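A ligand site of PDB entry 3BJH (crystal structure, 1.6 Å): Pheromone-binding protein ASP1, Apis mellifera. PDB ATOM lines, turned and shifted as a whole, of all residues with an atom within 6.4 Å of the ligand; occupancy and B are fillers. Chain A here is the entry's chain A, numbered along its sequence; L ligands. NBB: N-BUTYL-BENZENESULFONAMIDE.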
ATOM      1  N   VAL A   9      -4.565  11.606  25.463  1.00  0.00           N
ATOM      2  CA  VAL A   9      -5.928  11.152  25.180  1.00  0.00           C
ATOM      3  C   VAL A   9      -5.875  10.090  24.097  1.00  0.00           C
ATOM      4  O   VAL A   9      -6.718   9.190  24.065  1.00  0.00           O
ATOM      5  CB  VAL A   9      -6.821  12.324  24.769  1.00  0.00           C
ATOM      6  CG1 VAL A   9      -8.176  11.841  24.302  1.00  0.00           C
ATOM      7  CG2 VAL A   9      -6.946  13.325  25.928  1.00  0.00           C
ATOM      8  N   VAL A  13      -7.542   6.349  24.586  1.00  0.00           N
ATOM      9  CA  VAL A  13      -8.671   5.850  23.795  1.00  0.00           C
ATOM     10  C   VAL A  13      -8.324   4.749  22.786  1.00  0.00           C
ATOM     11  O   VAL A  13      -9.226   4.210  22.165  1.00  0.00           O
ATOM     12  CB  VAL A  13      -9.367   6.965  23.016  1.00  0.00           C
ATOM     13  CG1 VAL A  13      -9.913   8.044  23.955  1.00  0.00           C
ATOM     14  CG2 VAL A  13      -8.426   7.520  21.930  1.00  0.00           C
ATOM     15  N   TYR A  48     -19.730   5.162  15.016  1.00  0.00           N
ATOM     16  CA  TYR A  48     -18.417   5.287  15.641  1.00  0.00           C
ATOM     17  C   TYR A  48     -18.454   6.304  16.763  1.00  0.00           C
ATOM     18  O   TYR A  48     -17.963   6.042  17.870  1.00  0.00           O
ATOM     19  CB  TYR A  48     -17.327   5.687  14.607  1.00  0.00           C
ATOM     20  CG  TYR A  48     -16.005   5.998  15.240  1.00  0.00           C
ATOM     21  CD1 TYR A  48     -15.148   4.978  15.652  1.00  0.00           C
ATOM     22  CD2 TYR A  48     -15.638   7.282  15.501  1.00  0.00           C
ATOM     23  CE1 TYR A  48     -13.981   5.238  16.279  1.00  0.00           C
ATOM     24  CE2 TYR A  48     -14.470   7.565  16.147  1.00  0.00           C
ATOM     25  CZ  TYR A  48     -13.636   6.522  16.505  1.00  0.00           C
ATOM     26  OH  TYR A  48     -12.424   6.772  17.125  1.00  0.00           O
ATOM     27  N   MET A  49     -19.024   7.470  16.500  1.00  0.00           N
ATOM     28  CA  MET A  49     -19.089   8.476  17.543  1.00  0.00           C
ATOM     29  C   MET A  49     -19.915   8.002  18.737  1.00  0.00           C
ATOM     30  O   MET A  49     -19.526   8.162  19.878  1.00  0.00           O
ATOM     31  CB  MET A  49     -19.626   9.784  16.964  1.00  0.00           C
ATOM     32  CG  MET A  49     -18.675  10.403  15.931  1.00  0.00           C
ATOM     33  SD  MET A  49     -19.191  12.074  15.434  1.00  0.00           S
ATOM     34  CE  MET A  49     -20.611  11.734  14.442  1.00  0.00           C
ATOM     35  N   TYR A  50     -21.046   7.372  18.484  1.00  0.00           N
ATOM     36  CA  TYR A  50     -21.837   6.830  19.590  1.00  0.00           C
ATOM     37  C   TYR A  50     -21.012   5.810  20.369  1.00  0.00           C
ATOM     38  O   TYR A  50     -20.987   5.843  21.604  1.00  0.00           O
ATOM     39  CB  TYR A  50     -23.179   6.226  19.093  1.00  0.00           C
ATOM     40  CG  TYR A  50     -23.887   5.548  20.234  1.00  0.00           C
ATOM     41  CD1 TYR A  50     -24.625   6.284  21.133  1.00  0.00           C
ATOM     42  CD2 TYR A  50     -23.751   4.177  20.458  1.00  0.00           C
ATOM     43  CE1 TYR A  50     -25.199   5.680  22.263  1.00  0.00           C
ATOM     44  CE2 TYR A  50     -24.295   3.574  21.590  1.00  0.00           C
ATOM     45  CZ  TYR A  50     -25.046   4.328  22.468  1.00  0.00           C
ATOM     46  OH  TYR A  50     -25.601   3.700  23.590  1.00  0.00           O
ATOM     47  N   LEU A  52     -17.737   5.431  20.737  1.00  0.00           N
ATOM     48  CA  LEU A  52     -16.693   5.967  21.573  1.00  0.00           C
ATOM     49  C   LEU A  52     -17.256   6.737  22.768  1.00  0.00           C
ATOM     50  O   LEU A  52     -16.724   6.648  23.862  1.00  0.00           O
ATOM     51  CB  LEU A  52     -15.716   6.823  20.744  1.00  0.00           C
ATOM     52  CG  LEU A  52     -14.348   7.002  21.415  1.00  0.00           C
ATOM     53  CD1 LEU A  52     -13.611   5.672  21.561  1.00  0.00           C
ATOM     54  CD2 LEU A  52     -13.474   8.001  20.671  1.00  0.00           C
ATOM     55  N   LEU A  53     -18.328   7.478  22.568  1.00  0.00           N
ATOM     56  CA  LEU A  53     -18.981   8.196  23.679  1.00  0.00           C
ATOM     57  C   LEU A  53     -19.448   7.200  24.724  1.00  0.00           C
ATOM     58  O   LEU A  53     -19.282   7.379  25.910  1.00  0.00           O
ATOM     59  CB  LEU A  53     -20.182   8.982  23.137  1.00  0.00           C
ATOM     60  CG  LEU A  53     -19.831  10.261  22.398  1.00  0.00           C
ATOM     61  CD1 LEU A  53     -21.065  10.810  21.710  1.00  0.00           C
ATOM     62  CD2 LEU A  53     -19.216  11.299  23.341  1.00  0.00           C
ATOM     63  N   GLU A  54     -20.045   6.115  24.267  1.00  0.00           N
ATOM     64  CA  GLU A  54     -20.516   5.089  25.179  1.00  0.00           C
ATOM     65  C   GLU A  54     -19.394   4.453  25.955  1.00  0.00           C
ATOM     66  O   GLU A  54     -19.522   4.221  27.162  1.00  0.00           O
ATOM     67  CB  GLU A  54     -21.245   4.011  24.379  1.00  0.00           C
ATOM     68  CG  GLU A  54     -22.001   2.967  25.212  1.00  0.00           C
ATOM     69  CD  GLU A  54     -21.155   1.905  25.894  1.00  0.00           C
ATOM     70  OE1 GLU A  54     -20.125   1.458  25.364  1.00  0.00           O
ATOM     71  OE2 GLU A  54     -21.516   1.515  27.030  1.00  0.00           O
ATOM     72  N   PHE A  56     -16.793   5.719  27.067  1.00  0.00           N
ATOM     73  CA  PHE A  56     -16.351   6.582  28.158  1.00  0.00           C
ATOM     74  C   PHE A  56     -17.474   7.136  29.025  1.00  0.00           C
ATOM     75  O   PHE A  56     -17.286   8.117  29.750  1.00  0.00           O
ATOM     76  CB  PHE A  56     -15.438   7.660  27.611  1.00  0.00           C
ATOM     77  CG  PHE A  56     -14.102   7.114  27.228  1.00  0.00           C
ATOM     78  CD1 PHE A  56     -13.110   7.009  28.176  1.00  0.00           C
ATOM     79  CD2 PHE A  56     -13.877   6.643  25.949  1.00  0.00           C
ATOM     80  CE1 PHE A  56     -11.885   6.471  27.854  1.00  0.00           C
ATOM     81  CE2 PHE A  56     -12.647   6.085  25.616  1.00  0.00           C
ATOM     82  CZ  PHE A  56     -11.669   6.004  26.555  1.00  0.00           C
ATOM     83  N   LEU A  58     -20.253   8.663  28.350  1.00  0.00           N
ATOM     84  CA  LEU A  58     -20.731   9.986  28.062  1.00  0.00           C
ATOM     85  C   LEU A  58     -22.163   9.938  27.605  1.00  0.00           C
ATOM     86  O   LEU A  58     -22.858  10.952  27.682  1.00  0.00           O
ATOM     87  CB  LEU A  58     -19.850  10.636  27.012  1.00  0.00           C
ATOM     88  CG  LEU A  58     -18.503  11.041  27.612  1.00  0.00           C
ATOM     89  CD1 LEU A  58     -17.421  10.946  26.574  1.00  0.00           C
ATOM     90  CD2 LEU A  58     -18.648  12.429  28.168  1.00  0.00           C
ATOM     91  N   MET A  70     -19.573  15.118  30.200  1.00  0.00           N
ATOM     92  CA  MET A  70     -19.142  15.735  28.932  1.00  0.00           C
ATOM     93  C   MET A  70     -18.385  17.030  29.149  1.00  0.00           C
ATOM     94  O   MET A  70     -17.305  17.208  28.620  1.00  0.00           O
ATOM     95  CB  MET A  70     -20.313  15.989  27.983  1.00  0.00           C
ATOM     96  CG  MET A  70     -19.888  16.442  26.567  1.00  0.00           C
ATOM     97  SD  MET A  70     -21.094  16.067  25.252  1.00  0.00           S
ATOM     98  CE  MET A  70     -20.943  14.298  25.176  1.00  0.00           C
ATOM     99  N   LEU A  73     -14.877  16.561  30.326  1.00  0.00           N
ATOM    100  CA  LEU A  73     -13.874  16.261  29.304  1.00  0.00           C
ATOM    101  C   LEU A  73     -13.124  17.525  28.851  1.00  0.00           C
ATOM    102  O   LEU A  73     -11.939  17.471  28.563  1.00  0.00           O
ATOM    103  CB  LEU A  73     -14.507  15.603  28.075  1.00  0.00           C
ATOM    104  CG  LEU A  73     -14.339  14.110  27.832  1.00  0.00           C
ATOM    105  CD1 LEU A  73     -14.786  13.265  29.018  1.00  0.00           C
ATOM    106  CD2 LEU A  73     -15.101  13.737  26.577  1.00  0.00           C
ATOM    107  N   LEU A  74     -13.826  18.657  28.810  1.00  0.00           N
ATOM    108  CA  LEU A  74     -13.302  19.841  28.155  1.00  0.00           C
ATOM    109  C   LEU A  74     -12.409  20.642  29.120  1.00  0.00           C
ATOM    110  O   LEU A  74     -12.572  20.540  30.334  1.00  0.00           O
ATOM    111  CB  LEU A  74     -14.449  20.724  27.647  1.00  0.00           C
ATOM    112  CG  LEU A  74     -15.398  20.081  26.618  1.00  0.00           C
ATOM    113  CD1 LEU A  74     -16.601  20.994  26.305  1.00  0.00           C
ATOM    114  CD2 LEU A  74     -14.654  19.742  25.356  1.00  0.00           C
ATOM    115  N   MET A  86     -24.618  23.187  25.120  1.00  0.00           N
ATOM    116  CA  MET A  86     -25.429  22.031  25.567  1.00  0.00           C
ATOM    117  C   MET A  86     -26.854  22.433  25.917  1.00  0.00           C
ATOM    118  O   MET A  86     -27.778  21.637  25.778  1.00  0.00           O
ATOM    119  CB  MET A  86     -24.766  21.329  26.760  1.00  0.00           C
ATOM    120  CG  MET A  86     -23.382  20.763  26.436  1.00  0.00           C
ATOM    121  SD  MET A  86     -23.455  19.628  25.027  1.00  0.00           S
ATOM    122  CE  MET A  86     -21.728  19.249  24.755  1.00  0.00           C
ATOM    123  N   ILE A 101     -26.539  11.037  17.759  1.00  0.00           N
ATOM    124  CA  ILE A 101     -25.223  11.617  17.849  1.00  0.00           C
ATOM    125  C   ILE A 101     -24.858  12.429  16.594  1.00  0.00           C
ATOM    126  O   ILE A 101     -24.172  13.465  16.703  1.00  0.00           O
ATOM    127  CB  ILE A 101     -24.166  10.556  18.227  1.00  0.00           C
ATOM    128  CG1 ILE A 101     -24.540   9.863  19.549  1.00  0.00           C
ATOM    129  CG2 ILE A 101     -22.740  11.166  18.299  1.00  0.00           C
ATOM    130  CD1 ILE A 101     -24.828  10.798  20.753  1.00  0.00           C
ATOM    131  N   VAL A 108     -23.540  21.002  17.705  1.00  0.00           N
ATOM    132  CA  VAL A 108     -22.392  21.585  18.444  1.00  0.00           C
ATOM    133  C   VAL A 108     -21.466  22.272  17.466  1.00  0.00           C
ATOM    134  O   VAL A 108     -21.009  23.404  17.721  1.00  0.00           O
ATOM    135  CB  VAL A 108     -21.615  20.508  19.239  1.00  0.00           C
ATOM    136  CG1 VAL A 108     -20.350  21.068  19.876  1.00  0.00           C
ATOM    137  CG2 VAL A 108     -22.517  19.927  20.327  1.00  0.00           C
ATOM    138  N   VAL A 115     -15.431  22.966  20.066  1.00  0.00           N
ATOM    139  CA  VAL A 115     -16.014  22.128  21.110  1.00  0.00           C
ATOM    140  C   VAL A 115     -16.085  20.664  20.711  1.00  0.00           C
ATOM    141  O   VAL A 115     -15.532  19.813  21.401  1.00  0.00           O
ATOM    142  CB  VAL A 115     -17.386  22.673  21.549  1.00  0.00           C
ATOM    143  CG1 VAL A 115     -17.971  21.845  22.670  1.00  0.00           C
ATOM    144  CG2 VAL A 115     -17.239  24.137  21.979  1.00  0.00           C
ATOM    145  N   TRP A 116     -16.762  20.359  19.606  1.00  0.00           N
ATOM    146  CA  TRP A 116     -16.840  18.978  19.136  1.00  0.00           C
ATOM    147  C   TRP A 116     -15.507  18.569  18.548  1.00  0.00           C
ATOM    148  O   TRP A 116     -14.855  19.330  17.811  1.00  0.00           O
ATOM    149  CB  TRP A 116     -17.970  18.799  18.115  1.00  0.00           C
ATOM    150  CG  TRP A 116     -18.390  17.364  17.938  1.00  0.00           C
ATOM    151  CD1 TRP A 116     -18.016  16.514  16.931  1.00  0.00           C
ATOM    152  CD2 TRP A 116     -19.256  16.615  18.792  1.00  0.00           C
ATOM    153  NE1 TRP A 116     -18.598  15.292  17.118  1.00  0.00           N
ATOM    154  CE2 TRP A 116     -19.379  15.328  18.242  1.00  0.00           C
ATOM    155  CE3 TRP A 116     -19.964  16.924  19.967  1.00  0.00           C
ATOM    156  CZ2 TRP A 116     -20.161  14.333  18.832  1.00  0.00           C
ATOM    157  CZ3 TRP A 116     -20.751  15.927  20.549  1.00  0.00           C
ATOM    158  CH2 TRP A 116     -20.859  14.657  19.956  1.00  0.00           C
ATOM    159  N   PHE A 117     -15.047  17.393  18.943  1.00  0.00           N
ATOM    160  CA  PHE A 117     -13.806  16.836  18.416  1.00  0.00           C
ATOM    161  C   PHE A 117     -14.041  15.342  18.368  1.00  0.00           C
ATOM    162  O   PHE A 117     -14.782  14.802  19.183  1.00  0.00           O
ATOM    163  CB  PHE A 117     -12.602  17.199  19.300  1.00  0.00           C
ATOM    164  CG  PHE A 117     -12.607  16.529  20.646  1.00  0.00           C
ATOM    165  CD1 PHE A 117     -11.756  15.456  20.905  1.00  0.00           C
ATOM    166  CD2 PHE A 117     -13.435  16.981  21.669  1.00  0.00           C
ATOM    167  CE1 PHE A 117     -11.731  14.842  22.158  1.00  0.00           C
ATOM    168  CE2 PHE A 117     -13.437  16.374  22.915  1.00  0.00           C
ATOM    169  CZ  PHE A 117     -12.598  15.297  23.159  1.00  0.00           C
ATOM    170  N   VAL A 118     -13.442  14.687  17.388  1.00  0.00           N
ATOM    171  CA  VAL A 118     -13.562  13.245  17.300  1.00  0.00           C
ATOM    172  C   VAL A 118     -12.191  12.649  17.205  1.00  0.00           C
ATOM    173  O   VAL A 118     -11.421  13.048  16.340  1.00  0.00           O
ATOM    174  CB  VAL A 118     -14.423  12.833  16.097  1.00  0.00           C
ATOM    175  CG1 VAL A 118     -14.572  11.311  16.040  1.00  0.00           C
ATOM    176  CG2 VAL A 118     -15.765  13.510  16.159  1.00  0.00           C
ATOM    177  N   ILE A 119     -11.874  11.727  18.107  1.00  0.00           N
ATOM    178  CA  ILE A 119     -10.599  11.025  18.080  1.00  0.00           C
ATOM    179  C   ILE A 119     -10.773   9.682  17.402  1.00  0.00           C
ATOM    180  O   ILE A 119      -9.886   9.209  16.692  1.00  0.00           O
ATOM    181  CB  ILE A 119     -10.009  10.834  19.495  1.00  0.00           C
ATOM    182  CG1 ILE A 119      -9.389  12.134  19.994  1.00  0.00           C
ATOM    183  CG2 ILE A 119      -8.938   9.746  19.488  1.00  0.00           C
ATOM    184  CD1 ILE A 119      -8.397  11.954  21.107  1.00  0.00           C
ATOM    185  OXT ILE A 119     -11.837   9.072  17.536  1.00  0.00           O
HETATM  186  O1S NBB L   1     -17.047  10.655  20.110  1.00  0.00           O
HETATM  187  S   NBB L   1     -15.845  11.469  20.387  1.00  0.00           S
HETATM  188  O2S NBB L   1     -14.786  11.127  19.396  1.00  0.00           O
HETATM  189  N10 NBB L   1     -16.237  12.943  20.304  1.00  0.00           N
HETATM  190  C11 NBB L   1     -17.214  13.510  21.232  1.00  0.00           C
HETATM  191  C12 NBB L   1     -16.704  14.887  21.681  1.00  0.00           C
HETATM  192  C13 NBB L   1     -17.546  15.414  22.839  1.00  0.00           C
HETATM  193  C14 NBB L   1     -17.552  16.929  22.879  1.00  0.00           C
HETATM  194  C4  NBB L   1     -15.224  11.155  21.825  1.00  0.00           C
HETATM  195  C5  NBB L   1     -14.178  11.947  22.287  1.00  0.00           C
HETATM  196  C6  NBB L   1     -13.612  11.698  23.528  1.00  0.00           C
HETATM  197  C1  NBB L   1     -14.094  10.672  24.330  1.00  0.00           C
HETATM  198  C2  NBB L   1     -15.150   9.877  23.877  1.00  0.00           C
HETATM  199  C3  NBB L   1     -15.706  10.129  22.627  1.00  0.00           C
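An oxygen (O2S) of the ligand sits at hydrogen-bond distance from the backbone NH of Ile 119 (3.2 Å).
A nitrogen (N10) of the ligand sits at hydrogen-bond distance from the backbone carbonyl oxygen (O) of Phe 117.
The side-chain sulfur (SD) of Met 49 sits at hydrogen-bond distance from the indole nitrogen (NE1) of Trp 116 (3.7 Å).
The side-chain hydroxyl (OH) of Tyr 48 lies within hydrogen-bond range of the chain-end carboxylate (OXT) of Ile 119 (2.4 Å).
O of Leu 53 lies within hydrogen-bond range of N of Leu 58 (2.9 Å).
Merely in contact with the ligand: Met 49, Leu 52, Leu 53, Leu 58, Leu 73, Val 115, Trp 116 and Val 118.
Hydrophobic or aromatic side chains within 4 Å of the ligand: Leu 52, Leu 53, Leu 58, Leu 73, Trp 116, Phe 117 and Val 118.
Ten residues have an atom within 4 Å of the ligand: Met 49, Leu 52, Leu 53, Leu 58, Leu 73, Val 115, Trp 116, Phe 117, Val 118 and Ile 119.
The nearest printed residue that does not touch the ligand is Phe 56 (4.05 Å).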
